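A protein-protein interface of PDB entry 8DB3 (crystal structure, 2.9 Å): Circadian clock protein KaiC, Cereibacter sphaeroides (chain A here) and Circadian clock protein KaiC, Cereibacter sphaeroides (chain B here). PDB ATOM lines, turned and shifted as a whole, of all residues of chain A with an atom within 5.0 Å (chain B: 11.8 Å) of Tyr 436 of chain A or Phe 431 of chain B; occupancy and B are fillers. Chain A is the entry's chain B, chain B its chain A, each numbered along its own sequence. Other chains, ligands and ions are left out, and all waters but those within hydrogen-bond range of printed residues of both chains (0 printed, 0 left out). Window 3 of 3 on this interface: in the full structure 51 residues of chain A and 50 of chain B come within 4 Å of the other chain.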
ATOM      1  N   TRP A 419     -13.129 -11.306 -15.522  1.00  0.00           N
ATOM      2  CA  TRP A 419     -13.991 -12.412 -15.926  1.00  0.00           C
ATOM      3  C   TRP A 419     -13.191 -13.703 -15.969  1.00  0.00           C
ATOM      4  O   TRP A 419     -12.224 -13.811 -16.726  1.00  0.00           O
ATOM      5  CB  TRP A 419     -14.625 -12.127 -17.290  1.00  0.00           C
ATOM      6  CG  TRP A 419     -15.732 -13.059 -17.644  1.00  0.00           C
ATOM      7  CD1 TRP A 419     -16.374 -13.925 -16.808  1.00  0.00           C
ATOM      8  CD2 TRP A 419     -16.336 -13.223 -18.932  1.00  0.00           C
ATOM      9  NE1 TRP A 419     -17.339 -14.618 -17.494  1.00  0.00           N
ATOM     10  CE2 TRP A 419     -17.337 -14.206 -18.800  1.00  0.00           C
ATOM     11  CE3 TRP A 419     -16.127 -12.635 -20.182  1.00  0.00           C
ATOM     12  CZ2 TRP A 419     -18.125 -14.612 -19.870  1.00  0.00           C
ATOM     13  CZ3 TRP A 419     -16.912 -13.041 -21.243  1.00  0.00           C
ATOM     14  CH2 TRP A 419     -17.898 -14.020 -21.081  1.00  0.00           C
ATOM     15  N   VAL A 420     -13.615 -14.680 -15.170  1.00  0.00           N
ATOM     16  CA  VAL A 420     -12.984 -15.993 -15.093  1.00  0.00           C
ATOM     17  C   VAL A 420     -14.024 -17.033 -15.489  1.00  0.00           C
ATOM     18  O   VAL A 420     -15.098 -17.108 -14.880  1.00  0.00           O
ATOM     19  CB  VAL A 420     -12.432 -16.277 -13.686  1.00  0.00           C
ATOM     20  CG1 VAL A 420     -11.874 -17.689 -13.607  1.00  0.00           C
ATOM     21  CG2 VAL A 420     -11.368 -15.252 -13.317  1.00  0.00           C
ATOM     22  N   LEU A 421     -13.708 -17.829 -16.505  1.00  0.00           N
ATOM     23  CA  LEU A 421     -14.598 -18.872 -17.001  1.00  0.00           C
ATOM     24  C   LEU A 421     -14.043 -20.220 -16.562  1.00  0.00           C
ATOM     25  O   LEU A 421     -12.934 -20.598 -16.956  1.00  0.00           O
ATOM     26  CB  LEU A 421     -14.728 -18.805 -18.522  1.00  0.00           C
ATOM     27  CG  LEU A 421     -15.428 -19.964 -19.230  1.00  0.00           C
ATOM     28  CD1 LEU A 421     -16.935 -19.773 -19.221  1.00  0.00           C
ATOM     29  CD2 LEU A 421     -14.911 -20.097 -20.657  1.00  0.00           C
ATOM     30  N   LEU A 423     -14.460 -24.232 -16.557  1.00  0.00           N
ATOM     31  CA  LEU A 423     -15.056 -25.289 -17.357  1.00  0.00           C
ATOM     32  C   LEU A 423     -14.702 -26.645 -16.766  1.00  0.00           C
ATOM     33  O   LEU A 423     -13.575 -26.860 -16.320  1.00  0.00           O
ATOM     34  CB  LEU A 423     -14.575 -25.214 -18.808  1.00  0.00           C
ATOM     35  CG  LEU A 423     -14.677 -23.838 -19.467  1.00  0.00           C
ATOM     36  CD1 LEU A 423     -13.868 -23.794 -20.756  1.00  0.00           C
ATOM     37  CD2 LEU A 423     -16.137 -23.483 -19.722  1.00  0.00           C
ATOM     38  N   GLU A 434     -10.727 -26.711 -16.497  1.00  0.00           N
ATOM     39  CA  GLU A 434      -9.934 -25.666 -17.120  1.00  0.00           C
ATOM     40  C   GLU A 434     -10.411 -24.296 -16.666  1.00  0.00           C
ATOM     41  O   GLU A 434     -11.571 -24.109 -16.286  1.00  0.00           O
ATOM     42  CB  GLU A 434     -10.008 -25.766 -18.648  1.00  0.00           C
ATOM     43  CG  GLU A 434      -9.477 -27.078 -19.193  1.00  0.00           C
ATOM     44  CD  GLU A 434      -9.649 -27.200 -20.692  1.00  0.00           C
ATOM     45  OE1 GLU A 434     -10.507 -26.488 -21.254  1.00  0.00           O
ATOM     46  OE2 GLU A 434      -8.924 -28.012 -21.304  1.00  0.00           O
ATOM     47  N   LEU A 435      -9.493 -23.337 -16.715  1.00  0.00           N
ATOM     48  CA  LEU A 435      -9.727 -21.968 -16.288  1.00  0.00           C
ATOM     49  C   LEU A 435      -9.320 -21.048 -17.426  1.00  0.00           C
ATOM     50  O   LEU A 435      -8.225 -21.190 -17.987  1.00  0.00           O
ATOM     51  CB  LEU A 435      -8.932 -21.650 -15.017  1.00  0.00           C
ATOM     52  CG  LEU A 435      -8.870 -20.212 -14.507  1.00  0.00           C
ATOM     53  CD1 LEU A 435      -8.439 -20.212 -13.037  1.00  0.00           C
ATOM     54  CD2 LEU A 435      -7.924 -19.337 -15.305  1.00  0.00           C
ATOM     55  N   TYR A 436     -10.203 -20.103 -17.740  1.00  0.00           N
ATOM     56  CA  TYR A 436      -9.982 -19.077 -18.745  1.00  0.00           C
ATOM     57  C   TYR A 436     -10.002 -17.721 -18.050  1.00  0.00           C
ATOM     58  O   TYR A 436     -10.953 -17.415 -17.322  1.00  0.00           O
ATOM     59  CB  TYR A 436     -11.082 -19.095 -19.811  1.00  0.00           C
ATOM     60  CG  TYR A 436     -10.971 -20.134 -20.904  1.00  0.00           C
ATOM     61  CD1 TYR A 436     -10.215 -21.284 -20.746  1.00  0.00           C
ATOM     62  CD2 TYR A 436     -11.658 -19.963 -22.101  1.00  0.00           C
ATOM     63  CE1 TYR A 436     -10.149 -22.235 -21.754  1.00  0.00           C
ATOM     64  CE2 TYR A 436     -11.583 -20.897 -23.115  1.00  0.00           C
ATOM     65  CZ  TYR A 436     -10.820 -22.028 -22.942  1.00  0.00           C
ATOM     66  OH  TYR A 436     -10.749 -22.960 -23.954  1.00  0.00           O
ATOM     67  N   LEU A 437      -8.976 -16.908 -18.280  1.00  0.00           N
ATOM     68  CA  LEU A 437      -8.978 -15.509 -17.842  1.00  0.00           C
ATOM     69  C   LEU A 437      -9.365 -14.674 -19.062  1.00  0.00           C
ATOM     70  O   LEU A 437      -8.513 -14.256 -19.846  1.00  0.00           O
ATOM     71  CB  LEU A 437      -7.629 -15.103 -17.270  1.00  0.00           C
ATOM     72  CG  LEU A 437      -7.614 -13.766 -16.528  1.00  0.00           C
ATOM     73  CD1 LEU A 437      -8.523 -13.798 -15.309  1.00  0.00           C
ATOM     74  CD2 LEU A 437      -6.197 -13.408 -16.115  1.00  0.00           C
ATOM     75  N   LEU A 438     -10.669 -14.434 -19.218  1.00  0.00           N
ATOM     76  CA  LEU A 438     -11.165 -13.800 -20.435  1.00  0.00           C
ATOM     77  C   LEU A 438     -10.998 -12.284 -20.402  1.00  0.00           C
ATOM     78  O   LEU A 438     -10.685 -11.672 -21.429  1.00  0.00           O
ATOM     79  CB  LEU A 438     -12.638 -14.157 -20.649  1.00  0.00           C
ATOM     80  CG  LEU A 438     -12.987 -15.645 -20.662  1.00  0.00           C
ATOM     81  CD1 LEU A 438     -14.497 -15.850 -20.707  1.00  0.00           C
ATOM     82  CD2 LEU A 438     -12.311 -16.345 -21.832  1.00  0.00           C
ATOM     83  N   ASN A 447      -3.518 -14.873 -21.459  1.00  0.00           N
ATOM     84  CA  ASN A 447      -4.670 -15.342 -22.213  1.00  0.00           C
ATOM     85  C   ASN A 447      -4.601 -16.835 -22.503  1.00  0.00           C
ATOM     86  O   ASN A 447      -5.369 -17.331 -23.333  1.00  0.00           O
ATOM     87  CB  ASN A 447      -4.809 -14.552 -23.519  1.00  0.00           C
ATOM     88  CG  ASN A 447      -3.615 -14.715 -24.442  1.00  0.00           C
ATOM     89  OD1 ASN A 447      -2.638 -15.386 -24.111  1.00  0.00           O
ATOM     90  ND2 ASN A 447      -3.692 -14.094 -25.616  1.00  0.00           N
ATOM     91  N   GLN A 448      -3.696 -17.558 -21.843  1.00  0.00           N
ATOM     92  CA  GLN A 448      -3.647 -19.004 -21.979  1.00  0.00           C
ATOM     93  C   GLN A 448      -4.727 -19.645 -21.106  1.00  0.00           C
ATOM     94  O   GLN A 448      -5.297 -19.015 -20.210  1.00  0.00           O
ATOM     95  CB  GLN A 448      -2.276 -19.561 -21.586  1.00  0.00           C
ATOM     96  CG  GLN A 448      -1.075 -18.742 -22.041  1.00  0.00           C
ATOM     97  CD  GLN A 448      -0.265 -18.209 -20.874  1.00  0.00           C
ATOM     98  OE1 GLN A 448      -0.822 -17.771 -19.891  1.00  0.00           O
ATOM     99  NE2 GLN A 448       1.055 -18.259 -20.979  1.00  0.00           N
ATOM    100  N   VAL A 449      -4.994 -20.917 -21.380  1.00  0.00           N
ATOM    101  CA  VAL A 449      -5.999 -21.690 -20.661  1.00  0.00           C
ATOM    102  C   VAL A 449      -5.273 -22.632 -19.718  1.00  0.00           C
ATOM    103  O   VAL A 449      -4.381 -23.382 -20.138  1.00  0.00           O
ATOM    104  CB  VAL A 449      -6.905 -22.452 -21.642  1.00  0.00           C
ATOM    105  CG1 VAL A 449      -7.434 -21.486 -22.701  1.00  0.00           C
ATOM    106  CG2 VAL A 449      -6.170 -23.606 -22.308  1.00  0.00           C
ATOM    107  N   VAL B 273     -15.344  -9.505 -28.945  1.00  0.00           N
ATOM    108  CA  VAL B 273     -15.691 -10.078 -27.649  1.00  0.00           C
ATOM    109  C   VAL B 273     -15.114  -9.195 -26.551  1.00  0.00           C
ATOM    110  O   VAL B 273     -14.634  -8.086 -26.817  1.00  0.00           O
ATOM    111  CB  VAL B 273     -15.185 -11.526 -27.522  1.00  0.00           C
ATOM    112  CG1 VAL B 273     -15.800 -12.403 -28.609  1.00  0.00           C
ATOM    113  CG2 VAL B 273     -13.664 -11.577 -27.581  1.00  0.00           C
ATOM    114  N   ALA B 274     -15.156  -9.674 -25.310  1.00  0.00           N
ATOM    115  CA  ALA B 274     -14.589  -8.937 -24.189  1.00  0.00           C
ATOM    116  C   ALA B 274     -13.075  -9.105 -24.158  1.00  0.00           C
ATOM    117  O   ALA B 274     -12.548 -10.190 -24.423  1.00  0.00           O
ATOM    118  CB  ALA B 274     -15.195  -9.416 -22.869  1.00  0.00           C
ATOM    119  N   GLY B 275     -12.375  -8.022 -23.830  1.00  0.00           N
ATOM    120  CA  GLY B 275     -10.928  -8.043 -23.856  1.00  0.00           C
ATOM    121  C   GLY B 275     -10.331  -8.059 -25.241  1.00  0.00           C
ATOM    122  O   GLY B 275      -9.143  -8.355 -25.394  1.00  0.00           O
ATOM    123  N   ALA B 276     -11.129  -7.749 -26.264  1.00  0.00           N
ATOM    124  CA  ALA B 276     -10.632  -7.779 -27.633  1.00  0.00           C
ATOM    125  C   ALA B 276      -9.822  -6.536 -27.973  1.00  0.00           C
ATOM    126  O   ALA B 276      -8.902  -6.612 -28.795  1.00  0.00           O
ATOM    127  CB  ALA B 276     -11.801  -7.926 -28.610  1.00  0.00           C
ATOM    128  N   GLY B 277     -10.145  -5.397 -27.361  1.00  0.00           N
ATOM    129  CA  GLY B 277      -9.403  -4.174 -27.586  1.00  0.00           C
ATOM    130  C   GLY B 277     -10.249  -3.034 -28.112  1.00  0.00           C
ATOM    131  O   GLY B 277      -9.727  -2.086 -28.705  1.00  0.00           O
ATOM    132  N   MET B 422     -12.310  -7.087 -34.003  1.00  0.00           N
ATOM    133  CA  MET B 422     -11.164  -7.460 -33.183  1.00  0.00           C
ATOM    134  C   MET B 422     -11.434  -8.823 -32.562  1.00  0.00           C
ATOM    135  O   MET B 422     -12.417  -8.993 -31.832  1.00  0.00           O
ATOM    136  CB  MET B 422     -10.908  -6.406 -32.104  1.00  0.00           C
ATOM    137  CG  MET B 422     -11.114  -4.984 -32.601  1.00  0.00           C
ATOM    138  SD  MET B 422     -10.302  -3.711 -31.611  1.00  0.00           S
ATOM    139  CE  MET B 422      -8.614  -4.311 -31.552  1.00  0.00           C
ATOM    140  N   LEU B 423     -10.563  -9.789 -32.852  1.00  0.00           N
ATOM    141  CA  LEU B 423     -10.775 -11.174 -32.464  1.00  0.00           C
ATOM    142  C   LEU B 423      -9.753 -11.610 -31.423  1.00  0.00           C
ATOM    143  O   LEU B 423      -8.556 -11.339 -31.563  1.00  0.00           O
ATOM    144  CB  LEU B 423     -10.671 -12.102 -33.677  1.00  0.00           C
ATOM    145  CG  LEU B 423     -11.668 -11.924 -34.818  1.00  0.00           C
ATOM    146  CD1 LEU B 423     -11.862 -13.264 -35.521  1.00  0.00           C
ATOM    147  CD2 LEU B 423     -12.990 -11.379 -34.332  1.00  0.00           C
ATOM    148  N   ASN B 424     -10.234 -12.304 -30.398  1.00  0.00           N
ATOM    149  CA  ASN B 424      -9.400 -12.973 -29.400  1.00  0.00           C
ATOM    150  C   ASN B 424      -9.798 -14.449 -29.391  1.00  0.00           C
ATOM    151  O   ASN B 424     -10.460 -14.926 -28.465  1.00  0.00           O
ATOM    152  CB  ASN B 424      -9.573 -12.320 -28.021  1.00  0.00           C
ATOM    153  CG  ASN B 424      -8.358 -12.503 -27.129  1.00  0.00           C
ATOM    154  OD1 ASN B 424      -7.299 -12.941 -27.580  1.00  0.00           O
ATOM    155  ND2 ASN B 424      -8.506 -12.166 -25.852  1.00  0.00           N
ATOM    156  N   ARG B 425      -9.388 -15.174 -30.428  1.00  0.00           N
ATOM    157  CA  ARG B 425      -9.938 -16.493 -30.712  1.00  0.00           C
ATOM    158  C   ARG B 425      -9.057 -17.599 -30.149  1.00  0.00           C
ATOM    159  O   ARG B 425      -7.829 -17.521 -30.207  1.00  0.00           O
ATOM    160  CB  ARG B 425     -10.112 -16.688 -32.221  1.00  0.00           C
ATOM    161  CG  ARG B 425     -11.362 -16.030 -32.781  1.00  0.00           C
ATOM    162  CD  ARG B 425     -11.632 -16.485 -34.203  1.00  0.00           C
ATOM    163  NE  ARG B 425     -10.539 -16.134 -35.100  1.00  0.00           N
ATOM    164  CZ  ARG B 425     -10.588 -16.237 -36.420  1.00  0.00           C
ATOM    165  NH1 ARG B 425     -11.673 -16.671 -37.039  1.00  0.00           N
ATOM    166  NH2 ARG B 425      -9.520 -15.897 -37.138  1.00  0.00           N
ATOM    167  N   GLU B 426      -9.702 -18.635 -29.612  1.00  0.00           N
ATOM    168  CA  GLU B 426      -8.994 -19.762 -29.016  1.00  0.00           C
ATOM    169  C   GLU B 426      -8.333 -20.592 -30.110  1.00  0.00           C
ATOM    170  O   GLU B 426      -9.011 -21.093 -31.013  1.00  0.00           O
ATOM    171  CB  GLU B 426      -9.968 -20.605 -28.189  1.00  0.00           C
ATOM    172  CG  GLU B 426      -9.723 -22.117 -28.199  1.00  0.00           C
ATOM    173  CD  GLU B 426      -8.554 -22.537 -27.326  1.00  0.00           C
ATOM    174  OE1 GLU B 426      -8.185 -21.771 -26.413  1.00  0.00           O
ATOM    175  OE2 GLU B 426      -8.001 -23.634 -27.560  1.00  0.00           O
ATOM    176  N   VAL B 427      -7.014 -20.745 -30.024  1.00  0.00           N
ATOM    177  CA  VAL B 427      -6.266 -21.617 -30.920  1.00  0.00           C
ATOM    178  C   VAL B 427      -5.260 -22.391 -30.077  1.00  0.00           C
ATOM    179  O   VAL B 427      -4.438 -21.788 -29.378  1.00  0.00           O
ATOM    180  CB  VAL B 427      -5.555 -20.844 -32.046  1.00  0.00           C
ATOM    181  CG1 VAL B 427      -6.525 -19.878 -32.722  1.00  0.00           C
ATOM    182  CG2 VAL B 427      -4.332 -20.098 -31.528  1.00  0.00           C
ATOM    183  N   ASN B 428      -5.345 -23.720 -30.119  1.00  0.00           N
ATOM    184  CA  ASN B 428      -4.414 -24.583 -29.391  1.00  0.00           C
ATOM    185  C   ASN B 428      -4.344 -24.195 -27.915  1.00  0.00           C
ATOM    186  O   ASN B 428      -3.270 -24.118 -27.316  1.00  0.00           O
ATOM    187  CB  ASN B 428      -3.025 -24.538 -30.033  1.00  0.00           C
ATOM    188  CG  ASN B 428      -2.480 -25.920 -30.355  1.00  0.00           C
ATOM    189  OD1 ASN B 428      -2.949 -26.929 -29.825  1.00  0.00           O
ATOM    190  ND2 ASN B 428      -1.480 -25.971 -31.228  1.00  0.00           N
ATOM    191  N   GLY B 429      -5.508 -23.952 -27.318  1.00  0.00           N
ATOM    192  CA  GLY B 429      -5.552 -23.573 -25.918  1.00  0.00           C
ATOM    193  C   GLY B 429      -4.868 -22.261 -25.616  1.00  0.00           C
ATOM    194  O   GLY B 429      -4.320 -22.088 -24.521  1.00  0.00           O
ATOM    195  N   GLU B 430      -4.877 -21.329 -26.563  1.00  0.00           N
ATOM    196  CA  GLU B 430      -4.286 -20.013 -26.371  1.00  0.00           C
ATOM    197  C   GLU B 430      -5.029 -19.030 -27.262  1.00  0.00           C
ATOM    198  O   GLU B 430      -5.317 -19.333 -28.423  1.00  0.00           O
ATOM    199  CB  GLU B 430      -2.792 -20.010 -26.695  1.00  0.00           C
ATOM    200  CG  GLU B 430      -2.020 -18.858 -26.065  1.00  0.00           C
ATOM    201  CD  GLU B 430      -0.572 -18.811 -26.514  1.00  0.00           C
ATOM    202  OE1 GLU B 430      -0.247 -19.440 -27.542  1.00  0.00           O
ATOM    203  OE2 GLU B 430       0.241 -18.145 -25.839  1.00  0.00           O
ATOM    204  N   PHE B 431      -5.336 -17.857 -26.716  1.00  0.00           N
ATOM    205  CA  PHE B 431      -6.122 -16.861 -27.436  1.00  0.00           C
ATOM    206  C   PHE B 431      -5.195 -16.030 -28.320  1.00  0.00           C
ATOM    207  O   PHE B 431      -4.351 -15.281 -27.817  1.00  0.00           O
ATOM    208  CB  PHE B 431      -6.890 -15.975 -26.457  1.00  0.00           C
ATOM    209  CG  PHE B 431      -8.021 -16.680 -25.751  1.00  0.00           C
ATOM    210  CD1 PHE B 431      -8.231 -16.492 -24.394  1.00  0.00           C
ATOM    211  CD2 PHE B 431      -8.877 -17.523 -26.441  1.00  0.00           C
ATOM    212  CE1 PHE B 431      -9.269 -17.136 -23.741  1.00  0.00           C
ATOM    213  CE2 PHE B 431      -9.914 -18.168 -25.792  1.00  0.00           C
ATOM    214  CZ  PHE B 431     -10.109 -17.975 -24.442  1.00  0.00           C
ATOM    215  N   ASN B 432      -5.353 -16.165 -29.634  1.00  0.00           N
ATOM    216  CA  ASN B 432      -4.637 -15.346 -30.601  1.00  0.00           C
ATOM    217  C   ASN B 432      -5.461 -14.106 -30.931  1.00  0.00           C
ATOM    218  O   ASN B 432      -6.692 -14.170 -31.028  1.00  0.00           O
ATOM    219  CB  ASN B 432      -4.347 -16.139 -31.875  1.00  0.00           C
ATOM    220  N   ARG B 433      -4.767 -12.981 -31.109  1.00  0.00           N
ATOM    221  CA  ARG B 433      -5.388 -11.674 -31.291  1.00  0.00           C
ATOM    222  C   ARG B 433      -5.226 -11.225 -32.737  1.00  0.00           C
ATOM    223  O   ARG B 433      -4.105 -10.972 -33.193  1.00  0.00           O
ATOM    224  CB  ARG B 433      -4.767 -10.639 -30.345  1.00  0.00           C
ATOM    225  CG  ARG B 433      -4.947 -10.943 -28.865  1.00  0.00           C
ATOM    226  CD  ARG B 433      -4.959  -9.663 -28.031  1.00  0.00           C
ATOM    227  NE  ARG B 433      -6.001  -9.681 -27.010  1.00  0.00           N
ATOM    228  CZ  ARG B 433      -5.813  -9.376 -25.732  1.00  0.00           C
ATOM    229  NH1 ARG B 433      -4.619  -9.050 -25.266  1.00  0.00           N
ATOM    230  NH2 ARG B 433      -6.850  -9.398 -24.903  1.00  0.00           N
ATOM    231  N   GLU B 434      -6.349 -11.086 -33.438  1.00  0.00           N
ATOM    232  CA  GLU B 434      -6.356 -10.745 -34.854  1.00  0.00           C
ATOM    233  C   GLU B 434      -7.278  -9.558 -35.108  1.00  0.00           C
ATOM    234  O   GLU B 434      -8.101  -9.183 -34.266  1.00  0.00           O
ATOM    235  CB  GLU B 434      -6.796 -11.946 -35.708  1.00  0.00           C
ATOM    236  CG  GLU B 434      -6.258 -13.284 -35.225  1.00  0.00           C
ATOM    237  CD  GLU B 434      -6.745 -14.448 -36.068  1.00  0.00           C
ATOM    238  OE1 GLU B 434      -6.570 -14.401 -37.304  1.00  0.00           O
ATOM    239  OE2 GLU B 434      -7.303 -15.407 -35.496  1.00  0.00           O
ATOM    240  N   LEU B 435      -7.138  -8.975 -36.300  1.00  0.00           N
ATOM    241  CA  LEU B 435      -7.926  -7.819 -36.700  1.00  0.00           C
ATOM    242  C   LEU B 435      -8.383  -7.974 -38.141  1.00  0.00           C
ATOM    243  O   LEU B 435      -7.593  -8.366 -39.013  1.00  0.00           O
ATOM    244  CB  LEU B 435      -7.117  -6.524 -36.549  1.00  0.00           C
ATOM    245  CG  LEU B 435      -7.923  -5.229 -36.471  1.00  0.00           C
ATOM    246  CD1 LEU B 435      -8.785  -5.220 -35.221  1.00  0.00           C
ATOM    247  CD2 LEU B 435      -7.011  -4.015 -36.502  1.00  0.00           C
ATOM    248  N   ARG B 450      -4.903  -9.271 -40.029  1.00  0.00           N
ATOM    249  CA  ARG B 450      -3.641  -8.824 -39.447  1.00  0.00           C
ATOM    250  C   ARG B 450      -3.590  -9.199 -37.977  1.00  0.00           C
ATOM    251  O   ARG B 450      -4.416  -8.738 -37.186  1.00  0.00           O
ATOM    252  CB  ARG B 450      -3.460  -7.317 -39.643  1.00  0.00           C
ATOM    253  CG  ARG B 450      -3.410  -6.928 -41.114  1.00  0.00           C
ATOM    254  CD  ARG B 450      -2.517  -5.731 -41.360  1.00  0.00           C
ATOM    255  NE  ARG B 450      -1.097  -6.053 -41.311  1.00  0.00           N
ATOM    256  CZ  ARG B 450      -0.132  -5.146 -41.267  1.00  0.00           C
ATOM    257  NH1 ARG B 450      -0.403  -3.851 -41.257  1.00  0.00           N
ATOM    258  NH2 ARG B 450       1.135  -5.546 -41.232  1.00  0.00           N
ATOM    259  N   GLU B 451      -2.632 -10.049 -37.619  1.00  0.00           N
ATOM    260  CA  GLU B 451      -2.433 -10.393 -36.219  1.00  0.00           C
ATOM    261  C   GLU B 451      -1.840  -9.200 -35.483  1.00  0.00           C
ATOM    262  O   GLU B 451      -0.848  -8.607 -35.930  1.00  0.00           O
ATOM    263  CB  GLU B 451      -1.522 -11.607 -36.088  1.00  0.00           C
ATOM    264  CG  GLU B 451      -2.112 -12.876 -36.672  1.00  0.00           C
ATOM    265  CD  GLU B 451      -1.113 -14.012 -36.708  1.00  0.00           C
ATOM    266  OE1 GLU B 451      -0.021 -13.859 -36.119  1.00  0.00           O
ATOM    267  OE2 GLU B 451      -1.418 -15.055 -37.326  1.00  0.00           O
ATOM    268  N   PHE B 452      -2.446  -8.852 -34.350  1.00  0.00           N
ATOM    269  CA  PHE B 452      -2.071  -7.664 -33.603  1.00  0.00           C
ATOM    270  C   PHE B 452      -1.763  -8.026 -32.159  1.00  0.00           C
ATOM    271  O   PHE B 452      -2.379  -8.919 -31.572  1.00  0.00           O
ATOM    272  CB  PHE B 452      -3.176  -6.595 -33.664  1.00  0.00           C
ATOM    273  CG  PHE B 452      -4.298  -6.812 -32.687  1.00  0.00           C
ATOM    274  CD1 PHE B 452      -5.333  -7.684 -32.982  1.00  0.00           C
ATOM    275  CD2 PHE B 452      -4.329  -6.127 -31.485  1.00  0.00           C
ATOM    276  CE1 PHE B 452      -6.370  -7.876 -32.090  1.00  0.00           C
ATOM    277  CE2 PHE B 452      -5.362  -6.316 -30.589  1.00  0.00           C
ATOM    278  CZ  PHE B 452      -6.384  -7.191 -30.891  1.00  0.00           C
ATOM    279  N   LEU B 453      -0.794  -7.306 -31.603  1.00  0.00           N
ATOM    280  CA  LEU B 453      -0.305  -7.511 -30.251  1.00  0.00           C
ATOM    281  C   LEU B 453      -0.509  -6.248 -29.429  1.00  0.00           C
ATOM    282  O   LEU B 453      -0.260  -5.131 -29.904  1.00  0.00           O
ATOM    283  CB  LEU B 453       1.178  -7.895 -30.259  1.00  0.00           C
ATOM    284  CG  LEU B 453       1.880  -7.956 -28.903  1.00  0.00           C
ATOM    285  CD1 LEU B 453       1.259  -9.024 -28.014  1.00  0.00           C
ATOM    286  CD2 LEU B 453       3.373  -8.206 -29.096  1.00  0.00           C
ATOM    287  N   MET B 454      -0.968  -6.436 -28.195  1.00  0.00           N
ATOM    288  CA  MET B 454      -1.113  -5.361 -27.223  1.00  0.00           C
ATOM    289  C   MET B 454       0.081  -5.402 -26.277  1.00  0.00           C
ATOM    290  O   MET B 454       0.428  -6.466 -25.754  1.00  0.00           O
ATOM    291  CB  MET B 454      -2.422  -5.500 -26.446  1.00  0.00           C
ATOM    292  CG  MET B 454      -3.554  -4.641 -26.997  1.00  0.00           C
ATOM    293  SD  MET B 454      -5.033  -4.653 -25.974  1.00  0.00           S
ATOM    294  CE  MET B 454      -5.582  -6.333 -26.237  1.00  0.00           C
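O of Phe 431 of chain B lies within hydrogen-bond range of ND2 of Asn 447 of chain A.
The backbone carbonyl oxygen of Gly 429 of chain B sits close to the backbone NH of Val 449 of chain A (3.4 Å).
O of Trp 419 of chain A sits at hydrogen-bond distance from N of Leu 438 of chain A (3.0 Å).
N of Glu 430 of chain B is in hydrogen-bond range of OE1 of Glu 426 of chain B (3.3 Å).
The backbone NH of Tyr 436 of chain A is in hydrogen-bond range of the backbone carbonyl oxygen of Leu 421 of chain A (2.9 Å).
The backbone NH of Gly 429 of chain B lies within hydrogen-bond range of the side-chain carboxylate of Glu 426 of chain B (2.5 Å).
Among the printed residues, merely in contact across the chains: Tyr 436 of chain A with Glu 426 of chain B, Tyr 436 of chain A with Phe 431 of chain B, Leu 438 of chain A with Ala 274 of chain B, Leu 438 of chain A with Phe 431 of chain B and Val 449 of chain A with Glu 426 of chain B.
No residue of chain B comes within 4 Å of Val 420 of chain A.
No residue of chain B comes within 4 Å of Leu 421 of chain A.
No residue of chain B comes within 4 Å of Glu 434 of chain A.
No residue of chain B comes within 4 Å of Leu 435 of chain A.
Tyr 436 of chain A touches two residues of chain B.
Leu 437 of chain A touches none of the printed residues of chain B.
Leu 438 of chain A touches just these residues of chain B: Ala 274 and Phe 431.
Asn 447 of chain A touches one residue of chain B.
Val 449 of chain A touches just these residues of chain B: Glu 426 and Gly 429.
Of the printed residues of chain A, Ala 274 of chain B touches Leu 438 (3.8 Å).
Printed residues of chain A within 4 Å of Glu 426 of chain B: Tyr 436 (3.7 Å) and Val 449 (3.8 Å).
Printed residues of chain A within 4 Å of Gly 429 of chain B: Val 449 (3.3 Å).
Of chain A, only Tyr 436 (3.4 Å), Leu 438 (3.7 Å) and Asn 447 (2.6 Å) come within 4 Å of Phe 431 of chain B.
The nearest printed residue of chain A that does not touch Gly 429 of chain B is Gln 448 of chain A (4.1 Å).
Hydrophobic or aromatic side chains of chain A within 4 Å of the printed part of chain B: Tyr 436, Leu 438 and Val 449.
Of the 24 printed residues of chain B, 4 touch a printed residue of chain A.
Among the printed residues, no Asp or Glu carboxylate lies within 4 Å of a Lys or Arg side-chain nitrogen of the other chain.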
